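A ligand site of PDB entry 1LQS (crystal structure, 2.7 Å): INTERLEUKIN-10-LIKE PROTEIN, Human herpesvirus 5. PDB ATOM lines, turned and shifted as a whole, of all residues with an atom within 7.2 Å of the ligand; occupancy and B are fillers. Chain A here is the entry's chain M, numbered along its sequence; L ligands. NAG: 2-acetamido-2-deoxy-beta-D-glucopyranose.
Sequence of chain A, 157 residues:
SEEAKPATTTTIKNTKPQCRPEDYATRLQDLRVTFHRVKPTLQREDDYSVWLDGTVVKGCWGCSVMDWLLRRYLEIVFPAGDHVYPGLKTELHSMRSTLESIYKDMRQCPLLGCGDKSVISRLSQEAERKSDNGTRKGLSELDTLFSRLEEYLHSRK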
ATOM      1  N   GLU A 128      -3.933  11.748 -18.754  1.00  0.00           N
ATOM      2  CA  GLU A 128      -4.810  10.623 -18.478  1.00  0.00           C
ATOM      3  C   GLU A 128      -5.494  10.085 -19.732  1.00  0.00           C
ATOM      4  O   GLU A 128      -5.852   8.907 -19.797  1.00  0.00           O
ATOM      5  CB  GLU A 128      -5.866  10.997 -17.439  1.00  0.00           C
ATOM      6  CG  GLU A 128      -6.758   9.826 -17.019  1.00  0.00           C
ATOM      7  CD  GLU A 128      -5.966   8.697 -16.363  1.00  0.00           C
ATOM      8  OE1 GLU A 128      -4.955   8.249 -16.962  1.00  0.00           O
ATOM      9  OE2 GLU A 128      -6.362   8.239 -15.261  1.00  0.00           O
ATOM     10  N   LYS A 130      -4.357   9.208 -22.282  1.00  0.00           N
ATOM     11  CA  LYS A 130      -3.401   8.391 -23.016  1.00  0.00           C
ATOM     12  C   LYS A 130      -3.580   6.955 -22.551  1.00  0.00           C
ATOM     13  O   LYS A 130      -3.979   6.724 -21.414  1.00  0.00           O
ATOM     14  CB  LYS A 130      -1.965   8.855 -22.732  1.00  0.00           C
ATOM     15  CG  LYS A 130      -1.676  10.324 -23.019  1.00  0.00           C
ATOM     16  CD  LYS A 130      -1.696  10.643 -24.497  1.00  0.00           C
ATOM     17  CE  LYS A 130      -1.349  12.105 -24.746  1.00  0.00           C
ATOM     18  NZ  LYS A 130       0.005  12.487 -24.234  1.00  0.00           N
ATOM     19  N   SER A 131      -3.296   6.003 -23.424  1.00  0.00           N
ATOM     20  CA  SER A 131      -3.436   4.592 -23.101  1.00  0.00           C
ATOM     21  C   SER A 131      -2.480   4.066 -22.040  1.00  0.00           C
ATOM     22  O   SER A 131      -2.671   2.955 -21.549  1.00  0.00           O
ATOM     23  CB  SER A 131      -3.312   3.742 -24.371  1.00  0.00           C
ATOM     24  OG  SER A 131      -2.295   4.241 -25.217  1.00  0.00           O
ATOM     25  N   ASP A 132      -1.460   4.847 -21.684  1.00  0.00           N
ATOM     26  CA  ASP A 132      -0.507   4.420 -20.653  1.00  0.00           C
ATOM     27  C   ASP A 132      -0.360   5.502 -19.587  1.00  0.00           C
ATOM     28  O   ASP A 132       0.524   5.452 -18.731  1.00  0.00           O
ATOM     29  CB  ASP A 132       0.856   4.079 -21.284  1.00  0.00           C
ATOM     30  CG  ASP A 132       1.592   5.304 -21.814  1.00  0.00           C
ATOM     31  OD1 ASP A 132       0.961   6.384 -21.972  1.00  0.00           O
ATOM     32  OD2 ASP A 132       2.812   5.181 -22.088  1.00  0.00           O
ATOM     33  N   ASN A 133      -1.256   6.486 -19.662  1.00  0.00           N
ATOM     34  CA  ASN A 133      -1.317   7.601 -18.729  1.00  0.00           C
ATOM     35  C   ASN A 133      -0.232   8.669 -18.878  1.00  0.00           C
ATOM     36  O   ASN A 133       0.058   9.406 -17.938  1.00  0.00           O
ATOM     37  CB  ASN A 133      -1.337   7.089 -17.289  1.00  0.00           C
ATOM     38  CG  ASN A 133      -2.476   6.107 -17.061  1.00  0.00           C
ATOM     39  OD1 ASN A 133      -3.542   6.218 -17.669  1.00  0.00           O
ATOM     40  ND2 ASN A 133      -2.249   5.138 -16.174  1.00  0.00           N
ATOM     41  N   THR A 135       3.008   8.092 -19.600  1.00  0.00           N
ATOM     42  CA  THR A 135       4.372   7.661 -19.311  1.00  0.00           C
ATOM     43  C   THR A 135       5.244   7.886 -20.539  1.00  0.00           C
ATOM     44  O   THR A 135       6.299   8.481 -20.465  1.00  0.00           O
ATOM     45  CB  THR A 135       4.446   6.189 -18.901  1.00  0.00           C
ATOM     46  OG1 THR A 135       3.688   5.980 -17.697  1.00  0.00           O
ATOM     47  CG2 THR A 135       5.896   5.781 -18.644  1.00  0.00           C
HETATM   48  C1  NAG L   1      -5.156   3.949 -16.940  1.00  0.00           C
HETATM   49  C2  NAG L   1      -4.259   2.941 -16.123  1.00  0.00           C
HETATM   50  C3  NAG L   1      -5.225   2.188 -15.147  1.00  0.00           C
HETATM   51  C4  NAG L   1      -5.832   3.265 -14.210  1.00  0.00           C
HETATM   52  C5  NAG L   1      -6.663   4.303 -15.080  1.00  0.00           C
HETATM   53  C6  NAG L   1      -7.316   5.388 -14.295  1.00  0.00           C
HETATM   54  C7  NAG L   1      -2.311   1.765 -17.185  1.00  0.00           C
HETATM   55  C8  NAG L   1      -1.901   0.745 -18.137  1.00  0.00           C
HETATM   56  N2  NAG L   1      -3.672   1.950 -17.034  1.00  0.00           N
HETATM   57  O3  NAG L   1      -4.454   1.239 -14.382  1.00  0.00           O
HETATM   58  O4  NAG L   1      -6.723   2.630 -13.286  1.00  0.00           O
HETATM   59  O5  NAG L   1      -5.703   4.926 -16.039  1.00  0.00           O
HETATM   60  O6  NAG L   1      -8.349   6.025 -15.024  1.00  0.00           O
HETATM   61  O7  NAG L   1      -1.523   2.376 -16.600  1.00  0.00           O
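The nearest printed residue that does not touch the ligand is Ser 131 (4.1 Å).
OE2 of Glu 128 is in hydrogen-bond range of O6 of the ligand (3.0 Å).
The side-chain amide nitrogen of Asn 133 sits at hydrogen-bond distance from an oxygen (O7) of the ligand (2.9 Å).
The side-chain amide oxygen (OD1) of Asn 133 lies close to the side-chain carboxylate (OE1) of Glu 128, 2.6 Å away.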
